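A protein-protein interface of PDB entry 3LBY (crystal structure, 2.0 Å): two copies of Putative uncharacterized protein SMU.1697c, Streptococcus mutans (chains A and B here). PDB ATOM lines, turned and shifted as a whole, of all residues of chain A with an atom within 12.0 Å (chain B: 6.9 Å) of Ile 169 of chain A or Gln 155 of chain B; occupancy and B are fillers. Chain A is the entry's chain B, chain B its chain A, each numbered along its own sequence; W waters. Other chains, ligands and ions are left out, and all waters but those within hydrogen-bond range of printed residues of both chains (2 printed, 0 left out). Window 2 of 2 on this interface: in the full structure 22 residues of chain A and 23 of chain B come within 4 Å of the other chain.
The side-chain amide nitrogen (NE2) of Gln 156 of chain B lies within hydrogen-bond range of the side-chain carboxylate (OD1) of Asp 154 of chain B, at 2.8 Å. The side-chain carboxylate of Asp 154 of chain B sits at hydrogen-bond distance from a ring nitrogen (ND1) of His 157 of chain B (2.5 Å).
Of the 10 printed residues of chain B, 6 touch a printed residue of chain A. Printed residues of chain A that touch a printed residue of chain B: Ile 2, Pro 165, Leu 166, Asn 167, Gln 168 and Ile 169. Along chain A the printed residues that touch a printed residue of chain B span positions 2 to 169. Among the printed residues, 11 pairs touch across the chains. Among the printed residues, no Asp or Glu carboxylate lies within 4 Å of a Lys or Arg side-chain nitrogen of the other chain.
Of the printed residues of chain B, Pro 165 of chain A touches Val 160 (3.4 Å). Gln 155 of chain B touches just these residues of chain A: Asn 167, Gln 168 and Ile 169. No residue of chain A comes within 4 Å of His 157 of chain B. Printed residues of chain A within 4 Å of Phe 158 of chain B: Asn 167. Of chain A, only Ile 2 (3.97 Å) and Asn 167 (3.9 Å) come within 4 Å of Thr 159 of chain B. The nearest printed residue of chain B that does not touch Ile 169 of chain A is Gln 156 of chain B (7.0 Å). The nearest residue of chain A that does not touch Gln 155 of chain B is Asn 170 of chain A (4.7 Å). The nearest printed residue of chain A that does not touch Phe 158 of chain B is Gln 168 of chain A (6.0 Å).
No position is printed for both chains. Of the 11 pairs that touch across the chains among the printed residues, none has its exchanged pair printed and touching as well.
Water W1 lies within hydrogen-bond range of the backbone carbonyl oxygen (O) of Leu 153 of chain B and the backbone carbonyl oxygen (O) of Asn 167 of chain A. Water W2 bridges the backbone NH (N) of Asn 170 of chain A and the side-chain amide nitrogen (NE2) of Gln 155 of chain B.
The side-chain amide nitrogen of Gln 155 of chain B sits close to the backbone NH of Ile 169 of chain A (2.8 Å). The backbone carbonyl oxygen (O) of Val 160 of chain B sits at hydrogen-bond distance from the backbone NH (N) of Leu 166 of chain A, at 2.8 Å. The side-chain amide nitrogen of Asn 167 of chain A is in hydrogen-bond range of the backbone carbonyl oxygen of Phe 158 of chain B, 2.8 Å away. O of Leu 153 of chain B sits at hydrogen-bond distance from ND2 of Asn 167 of chain A (2.9 Å). The side-chain amide oxygen (OD1) of Asn 167 of chain A sits at hydrogen-bond distance from the backbone NH (N) of Val 160 of chain B, 2.9 Å away.
Among the printed residues, merely in contact across the chains: Pro 165 of chain A with Val 160 of chain B, Gln 168 of chain A with Gln 155 of chain B, Asn 167 of chain A with Gln 155 of chain B, Asn 167 of chain A with Asp 154 of chain B, Asn 167 of chain A with Thr 159 of chain B and Ile 2 of chain A with Thr 159 of chain B.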
ATOM      1  N   MET A   1     -22.208  25.268 -13.071  1.00  0.00           N
ATOM      2  CA  MET A   1     -22.142  26.639 -12.583  1.00  0.00           C
ATOM      3  C   MET A   1     -20.915  26.873 -11.713  1.00  0.00           C
ATOM      4  O   MET A   1     -20.429  27.997 -11.633  1.00  0.00           O
ATOM      5  CB  MET A   1     -23.403  27.013 -11.809  1.00  0.00           C
ATOM      6  CG  MET A   1     -23.522  28.500 -11.511  1.00  0.00           C
ATOM      7  SD  MET A   1     -24.455  28.839 -10.008  1.00  0.00           S
ATOM      8  CE  MET A   1     -25.828  27.704 -10.192  1.00  0.00           C
ATOM      9  N   ILE A   2     -20.416  25.827 -11.058  1.00  0.00           N
ATOM     10  CA  ILE A   2     -19.148  25.947 -10.344  1.00  0.00           C
ATOM     11  C   ILE A   2     -18.112  26.440 -11.337  1.00  0.00           C
ATOM     12  O   ILE A   2     -18.090  25.992 -12.479  1.00  0.00           O
ATOM     13  CB  ILE A   2     -18.631  24.604  -9.803  1.00  0.00           C
ATOM     14  CG1 ILE A   2     -19.470  24.105  -8.639  1.00  0.00           C
ATOM     15  CG2 ILE A   2     -17.209  24.758  -9.291  1.00  0.00           C
ATOM     16  CD1 ILE A   2     -18.801  22.961  -7.892  1.00  0.00           C
ATOM     17  N   ARG A   4     -14.770  26.822 -13.399  1.00  0.00           N
ATOM     18  CA  ARG A   4     -13.562  26.100 -13.768  1.00  0.00           C
ATOM     19  C   ARG A   4     -12.381  26.957 -13.321  1.00  0.00           C
ATOM     20  O   ARG A   4     -12.503  28.173 -13.237  1.00  0.00           O
ATOM     21  CB  ARG A   4     -13.500  25.869 -15.277  1.00  0.00           C
ATOM     22  CG  ARG A   4     -14.485  24.811 -15.808  1.00  0.00           C
ATOM     23  CD  ARG A   4     -14.269  24.578 -17.300  1.00  0.00           C
ATOM     24  NE  ARG A   4     -14.356  25.827 -18.056  1.00  0.00           N
ATOM     25  CZ  ARG A   4     -13.596  26.126 -19.110  1.00  0.00           C
ATOM     26  NH1 ARG A   4     -12.679  25.268 -19.536  1.00  0.00           N
ATOM     27  NH2 ARG A   4     -13.747  27.289 -19.732  1.00  0.00           N
ATOM     28  N   PRO A   5     -11.244  26.316 -13.016  1.00  0.00           N
ATOM     29  CA  PRO A   5     -10.016  27.011 -12.630  1.00  0.00           C
ATOM     30  C   PRO A   5      -9.665  28.173 -13.563  1.00  0.00           C
ATOM     31  O   PRO A   5      -9.327  29.258 -13.081  1.00  0.00           O
ATOM     32  CB  PRO A   5      -8.961  25.904 -12.701  1.00  0.00           C
ATOM     33  CG  PRO A   5      -9.755  24.645 -12.364  1.00  0.00           C
ATOM     34  CD  PRO A   5     -11.060  24.851 -13.063  1.00  0.00           C
ATOM     35  N   GLN A 164      -8.567  23.155  -7.292  1.00  0.00           N
ATOM     36  CA  GLN A 164      -8.235  22.008  -8.123  1.00  0.00           C
ATOM     37  C   GLN A 164      -9.392  21.023  -8.276  1.00  0.00           C
ATOM     38  O   GLN A 164      -9.968  20.597  -7.281  1.00  0.00           O
ATOM     39  CB  GLN A 164      -7.062  21.284  -7.492  1.00  0.00           C
ATOM     40  CG  GLN A 164      -6.501  20.174  -8.327  1.00  0.00           C
ATOM     41  CD  GLN A 164      -5.358  19.489  -7.629  1.00  0.00           C
ATOM     42  OE1 GLN A 164      -5.485  19.072  -6.479  1.00  0.00           O
ATOM     43  NE2 GLN A 164      -4.225  19.376  -8.314  1.00  0.00           N
ATOM     44  N   PRO A 165      -9.716  20.647  -9.525  1.00  0.00           N
ATOM     45  CA  PRO A 165     -10.747  19.634  -9.786  1.00  0.00           C
ATOM     46  C   PRO A 165     -10.260  18.301  -9.247  1.00  0.00           C
ATOM     47  O   PRO A 165      -9.090  17.988  -9.404  1.00  0.00           O
ATOM     48  CB  PRO A 165     -10.811  19.566 -11.324  1.00  0.00           C
ATOM     49  CG  PRO A 165     -10.059  20.744 -11.820  1.00  0.00           C
ATOM     50  CD  PRO A 165      -9.061  21.105 -10.761  1.00  0.00           C
ATOM     51  N   LEU A 166     -11.134  17.531  -8.617  1.00  0.00           N
ATOM     52  CA  LEU A 166     -10.717  16.274  -8.015  1.00  0.00           C
ATOM     53  C   LEU A 166     -11.194  15.043  -8.783  1.00  0.00           C
ATOM     54  O   LEU A 166     -10.588  13.983  -8.668  1.00  0.00           O
ATOM     55  CB  LEU A 166     -11.215  16.179  -6.569  1.00  0.00           C
ATOM     56  CG  LEU A 166     -10.617  17.195  -5.591  1.00  0.00           C
ATOM     57  CD1 LEU A 166     -11.194  16.994  -4.180  1.00  0.00           C
ATOM     58  CD2 LEU A 166      -9.096  17.093  -5.590  1.00  0.00           C
ATOM     59  N   ASN A 167     -12.284  15.169  -9.536  1.00  0.00           N
ATOM     60  CA  ASN A 167     -12.894  13.988 -10.153  1.00  0.00           C
ATOM     61  C   ASN A 167     -12.889  13.971 -11.682  1.00  0.00           C
ATOM     62  O   ASN A 167     -13.709  13.292 -12.296  1.00  0.00           O
ATOM     63  CB  ASN A 167     -14.315  13.733  -9.613  1.00  0.00           C
ATOM     64  CG  ASN A 167     -15.330  14.727 -10.135  1.00  0.00           C
ATOM     65  OD1 ASN A 167     -15.042  15.923 -10.250  1.00  0.00           O
ATOM     66  ND2 ASN A 167     -16.533  14.238 -10.459  1.00  0.00           N
ATOM     67  N   GLN A 168     -11.969  14.714 -12.291  1.00  0.00           N
ATOM     68  CA  GLN A 168     -11.846  14.727 -13.755  1.00  0.00           C
ATOM     69  C   GLN A 168     -11.008  13.552 -14.230  1.00  0.00           C
ATOM     70  O   GLN A 168      -9.975  13.254 -13.647  1.00  0.00           O
ATOM     71  CB  GLN A 168     -11.230  16.040 -14.230  1.00  0.00           C
ATOM     72  CG  GLN A 168     -12.150  17.242 -14.068  1.00  0.00           C
ATOM     73  CD  GLN A 168     -13.013  17.458 -15.287  1.00  0.00           C
ATOM     74  OE1 GLN A 168     -14.205  17.149 -15.285  1.00  0.00           O
ATOM     75  NE2 GLN A 168     -12.406  17.973 -16.356  1.00  0.00           N
ATOM     76  N   ILE A 169     -11.452  12.887 -15.292  1.00  0.00           N
ATOM     77  CA  ILE A 169     -10.795  11.663 -15.730  1.00  0.00           C
ATOM     78  C   ILE A 169      -9.479  11.930 -16.462  1.00  0.00           C
ATOM     79  O   ILE A 169      -8.499  11.210 -16.257  1.00  0.00           O
ATOM     80  CB  ILE A 169     -11.730  10.790 -16.584  1.00  0.00           C
ATOM     81  CG1 ILE A 169     -11.286   9.326 -16.528  1.00  0.00           C
ATOM     82  CG2 ILE A 169     -11.793  11.302 -18.014  1.00  0.00           C
ATOM     83  CD1 ILE A 169     -10.167   8.974 -17.486  1.00  0.00           C
ATOM     84  N   ASN A 170      -9.461  12.959 -17.307  1.00  0.00           N
ATOM     85  CA  ASN A 170      -8.222  13.410 -17.935  1.00  0.00           C
ATOM     86  C   ASN A 170      -7.637  14.486 -17.020  1.00  0.00           C
ATOM     87  O   ASN A 170      -8.358  15.381 -16.584  1.00  0.00           O
ATOM     88  CB  ASN A 170      -8.484  13.944 -19.360  1.00  0.00           C
ATOM     89  CG  ASN A 170      -8.974  12.855 -20.321  1.00  0.00           C
ATOM     90  OD1 ASN A 170      -8.440  11.747 -20.336  1.00  0.00           O
ATOM     91  ND2 ASN A 170      -9.990  13.175 -21.133  1.00  0.00           N
ATOM     92  N   THR A 171      -6.350  14.394 -16.702  1.00  0.00           N
ATOM     93  CA  THR A 171      -5.768  15.296 -15.712  1.00  0.00           C
ATOM     94  C   THR A 171      -5.855  16.752 -16.153  1.00  0.00           C
ATOM     95  O   THR A 171      -5.153  17.188 -17.057  1.00  0.00           O
ATOM     96  CB  THR A 171      -4.332  14.905 -15.323  1.00  0.00           C
ATOM     97  OG1 THR A 171      -3.514  14.830 -16.494  1.00  0.00           O
ATOM     98  CG2 THR A 171      -4.333  13.551 -14.631  1.00  0.00           C
ATOM     99  N   PRO A 172      -6.737  17.513 -15.497  1.00  0.00           N
ATOM    100  CA  PRO A 172      -7.065  18.877 -15.899  1.00  0.00           C
ATOM    101  C   PRO A 172      -6.117  19.899 -15.275  1.00  0.00           C
ATOM    102  O   PRO A 172      -5.322  19.565 -14.395  1.00  0.00           O
ATOM    103  CB  PRO A 172      -8.464  19.041 -15.319  1.00  0.00           C
ATOM    104  CG  PRO A 172      -8.338  18.358 -13.989  1.00  0.00           C
ATOM    105  CD  PRO A 172      -7.418  17.156 -14.238  1.00  0.00           C
ATOM    106  N   PRO A 173      -6.199  21.146 -15.740  1.00  0.00           N
ATOM    107  CA  PRO A 173      -5.379  22.233 -15.202  1.00  0.00           C
ATOM    108  C   PRO A 173      -5.876  22.610 -13.814  1.00  0.00           C
ATOM    109  O   PRO A 173      -7.052  22.415 -13.529  1.00  0.00           O
ATOM    110  CB  PRO A 173      -5.655  23.390 -16.168  1.00  0.00           C
ATOM    111  CG  PRO A 173      -6.276  22.749 -17.398  1.00  0.00           C
ATOM    112  CD  PRO A 173      -7.020  21.576 -16.884  1.00  0.00           C
ATOM    113  N   GLU B 152     -13.737   9.649  -6.970  1.00  0.00           N
ATOM    114  CA  GLU B 152     -14.301   8.605  -7.838  1.00  0.00           C
ATOM    115  C   GLU B 152     -15.708   8.944  -8.338  1.00  0.00           C
ATOM    116  O   GLU B 152     -16.287   8.204  -9.132  1.00  0.00           O
ATOM    117  CB  GLU B 152     -14.301   7.238  -7.143  1.00  0.00           C
ATOM    118  CG  GLU B 152     -12.942   6.780  -6.630  1.00  0.00           C
ATOM    119  CD  GLU B 152     -11.961   6.474  -7.744  1.00  0.00           C
ATOM    120  OE1 GLU B 152     -12.398   6.333  -8.905  1.00  0.00           O
ATOM    121  OE2 GLU B 152     -10.749   6.370  -7.460  1.00  0.00           O
ATOM    122  N   LEU B 153     -16.271  10.050  -7.863  1.00  0.00           N
ATOM    123  CA  LEU B 153     -17.564  10.488  -8.369  1.00  0.00           C
ATOM    124  C   LEU B 153     -17.469  10.710  -9.872  1.00  0.00           C
ATOM    125  O   LEU B 153     -16.506  11.305 -10.357  1.00  0.00           O
ATOM    126  CB  LEU B 153     -18.016  11.760  -7.665  1.00  0.00           C
ATOM    127  CG  LEU B 153     -18.438  11.545  -6.212  1.00  0.00           C
ATOM    128  CD1 LEU B 153     -18.577  12.883  -5.484  1.00  0.00           C
ATOM    129  CD2 LEU B 153     -19.741  10.713  -6.127  1.00  0.00           C
ATOM    130  N   ASP B 154     -18.461  10.214 -10.606  1.00  0.00           N
ATOM    131  CA  ASP B 154     -18.465  10.305 -12.065  1.00  0.00           C
ATOM    132  C   ASP B 154     -18.569  11.762 -12.503  1.00  0.00           C
ATOM    133  O   ASP B 154     -19.449  12.493 -12.040  1.00  0.00           O
ATOM    134  CB  ASP B 154     -19.631   9.479 -12.644  1.00  0.00           C
ATOM    135  CG  ASP B 154     -19.771   9.645 -14.142  1.00  0.00           C
ATOM    136  OD1 ASP B 154     -18.821   9.298 -14.868  1.00  0.00           O
ATOM    137  OD2 ASP B 154     -20.827  10.130 -14.599  1.00  0.00           O
ATOM    138  N   GLN B 155     -17.671  12.186 -13.393  1.00  0.00           N
ATOM    139  CA  GLN B 155     -17.586  13.589 -13.792  1.00  0.00           C
ATOM    140  C   GLN B 155     -18.787  14.066 -14.600  1.00  0.00           C
ATOM    141  O   GLN B 155     -19.095  15.255 -14.625  1.00  0.00           O
ATOM    142  CB  GLN B 155     -16.285  13.876 -14.565  1.00  0.00           C
ATOM    143  CG  GLN B 155     -16.366  13.636 -16.048  1.00  0.00           C
ATOM    144  CD  GLN B 155     -15.135  14.134 -16.787  1.00  0.00           C
ATOM    145  OE1 GLN B 155     -15.240  14.848 -17.788  1.00  0.00           O
ATOM    146  NE2 GLN B 155     -13.963  13.752 -16.304  1.00  0.00           N
ATOM    147  N   GLN B 156     -19.463  13.141 -15.269  1.00  0.00           N
ATOM    148  CA  GLN B 156     -20.692  13.473 -15.967  1.00  0.00           C
ATOM    149  C   GLN B 156     -21.850  13.761 -15.000  1.00  0.00           C
ATOM    150  O   GLN B 156     -22.813  14.436 -15.369  1.00  0.00           O
ATOM    151  CB  GLN B 156     -21.058  12.333 -16.914  1.00  0.00           C
ATOM    152  CG  GLN B 156     -20.106  12.224 -18.099  1.00  0.00           C
ATOM    153  CD  GLN B 156     -19.604  10.810 -18.324  1.00  0.00           C
ATOM    154  OE1 GLN B 156     -20.001  10.139 -19.282  1.00  0.00           O
ATOM    155  NE2 GLN B 156     -18.724  10.347 -17.438  1.00  0.00           N
ATOM    156  N   HIS B 157     -21.764  13.258 -13.771  1.00  0.00           N
ATOM    157  CA  HIS B 157     -22.844  13.488 -12.795  1.00  0.00           C
ATOM    158  C   HIS B 157     -22.504  14.464 -11.673  1.00  0.00           C
ATOM    159  O   HIS B 157     -23.411  15.050 -11.045  1.00  0.00           O
ATOM    160  CB  HIS B 157     -23.344  12.165 -12.225  1.00  0.00           C
ATOM    161  CG  HIS B 157     -23.999  11.291 -13.253  1.00  0.00           C
ATOM    162  ND1 HIS B 157     -23.283  10.506 -14.123  1.00  0.00           N
ATOM    163  CD2 HIS B 157     -25.304  11.115 -13.574  1.00  0.00           C
ATOM    164  CE1 HIS B 157     -24.114   9.863 -14.928  1.00  0.00           C
ATOM    165  NE2 HIS B 157     -25.346  10.216 -14.612  1.00  0.00           N
ATOM    166  N   PHE B 158     -21.211  14.635 -11.404  1.00  0.00           N
ATOM    167  CA  PHE B 158     -20.777  15.547 -10.337  1.00  0.00           C
ATOM    168  C   PHE B 158     -19.502  16.307 -10.730  1.00  0.00           C
ATOM    169  O   PHE B 158     -18.622  15.766 -11.397  1.00  0.00           O
ATOM    170  CB  PHE B 158     -20.525  14.792  -9.022  1.00  0.00           C
ATOM    171  CG  PHE B 158     -21.729  14.058  -8.506  1.00  0.00           C
ATOM    172  CD1 PHE B 158     -22.630  14.683  -7.657  1.00  0.00           C
ATOM    173  CD2 PHE B 158     -21.973  12.743  -8.891  1.00  0.00           C
ATOM    174  CE1 PHE B 158     -23.755  13.999  -7.194  1.00  0.00           C
ATOM    175  CE2 PHE B 158     -23.093  12.054  -8.419  1.00  0.00           C
ATOM    176  CZ  PHE B 158     -23.981  12.692  -7.573  1.00  0.00           C
ATOM    177  N   THR B 159     -19.435  17.569 -10.323  1.00  0.00           N
ATOM    178  CA  THR B 159     -18.218  18.359 -10.448  1.00  0.00           C
ATOM    179  C   THR B 159     -17.658  18.532  -9.042  1.00  0.00           C
ATOM    180  O   THR B 159     -18.365  19.021  -8.143  1.00  0.00           O
ATOM    181  CB  THR B 159     -18.505  19.736 -11.054  1.00  0.00           C
ATOM    182  OG1 THR B 159     -18.971  19.574 -12.398  1.00  0.00           O
ATOM    183  CG2 THR B 159     -17.230  20.609 -11.043  1.00  0.00           C
ATOM    184  N   VAL B 160     -16.414  18.105  -8.835  1.00  0.00           N
ATOM    185  CA  VAL B 160     -15.812  18.153  -7.498  1.00  0.00           C
ATOM    186  C   VAL B 160     -14.565  19.029  -7.499  1.00  0.00           C
ATOM    187  O   VAL B 160     -13.624  18.766  -8.252  1.00  0.00           O
ATOM    188  CB  VAL B 160     -15.411  16.754  -6.999  1.00  0.00           C
ATOM    189  CG1 VAL B 160     -14.855  16.838  -5.579  1.00  0.00           C
ATOM    190  CG2 VAL B 160     -16.611  15.797  -7.049  1.00  0.00           C
ATOM    191  N   LEU B 181     -24.734  17.510 -11.389  1.00  0.00           N
ATOM    192  CA  LEU B 181     -24.957  17.901 -12.768  1.00  0.00           C
ATOM    193  C   LEU B 181     -26.245  17.272 -13.305  1.00  0.00           C
ATOM    194  O   LEU B 181     -26.834  17.765 -14.264  1.00  0.00           O
ATOM    195  CB  LEU B 181     -23.785  17.435 -13.631  1.00  0.00           C
ATOM    196  CG  LEU B 181     -22.540  18.316 -13.810  1.00  0.00           C
ATOM    197  CD1 LEU B 181     -22.357  19.300 -12.698  1.00  0.00           C
ATOM    198  CD2 LEU B 181     -21.278  17.469 -14.011  1.00  0.00           C
ATOM    199  OXT LEU B 181     -26.715  16.257 -12.801  1.00  0.00           O
HETATM  200  O   HOH W   1     -13.996  10.120 -11.361  1.00  0.00           O
HETATM  201  O   HOH W   2     -11.597  15.014 -18.136  1.00  0.00           O
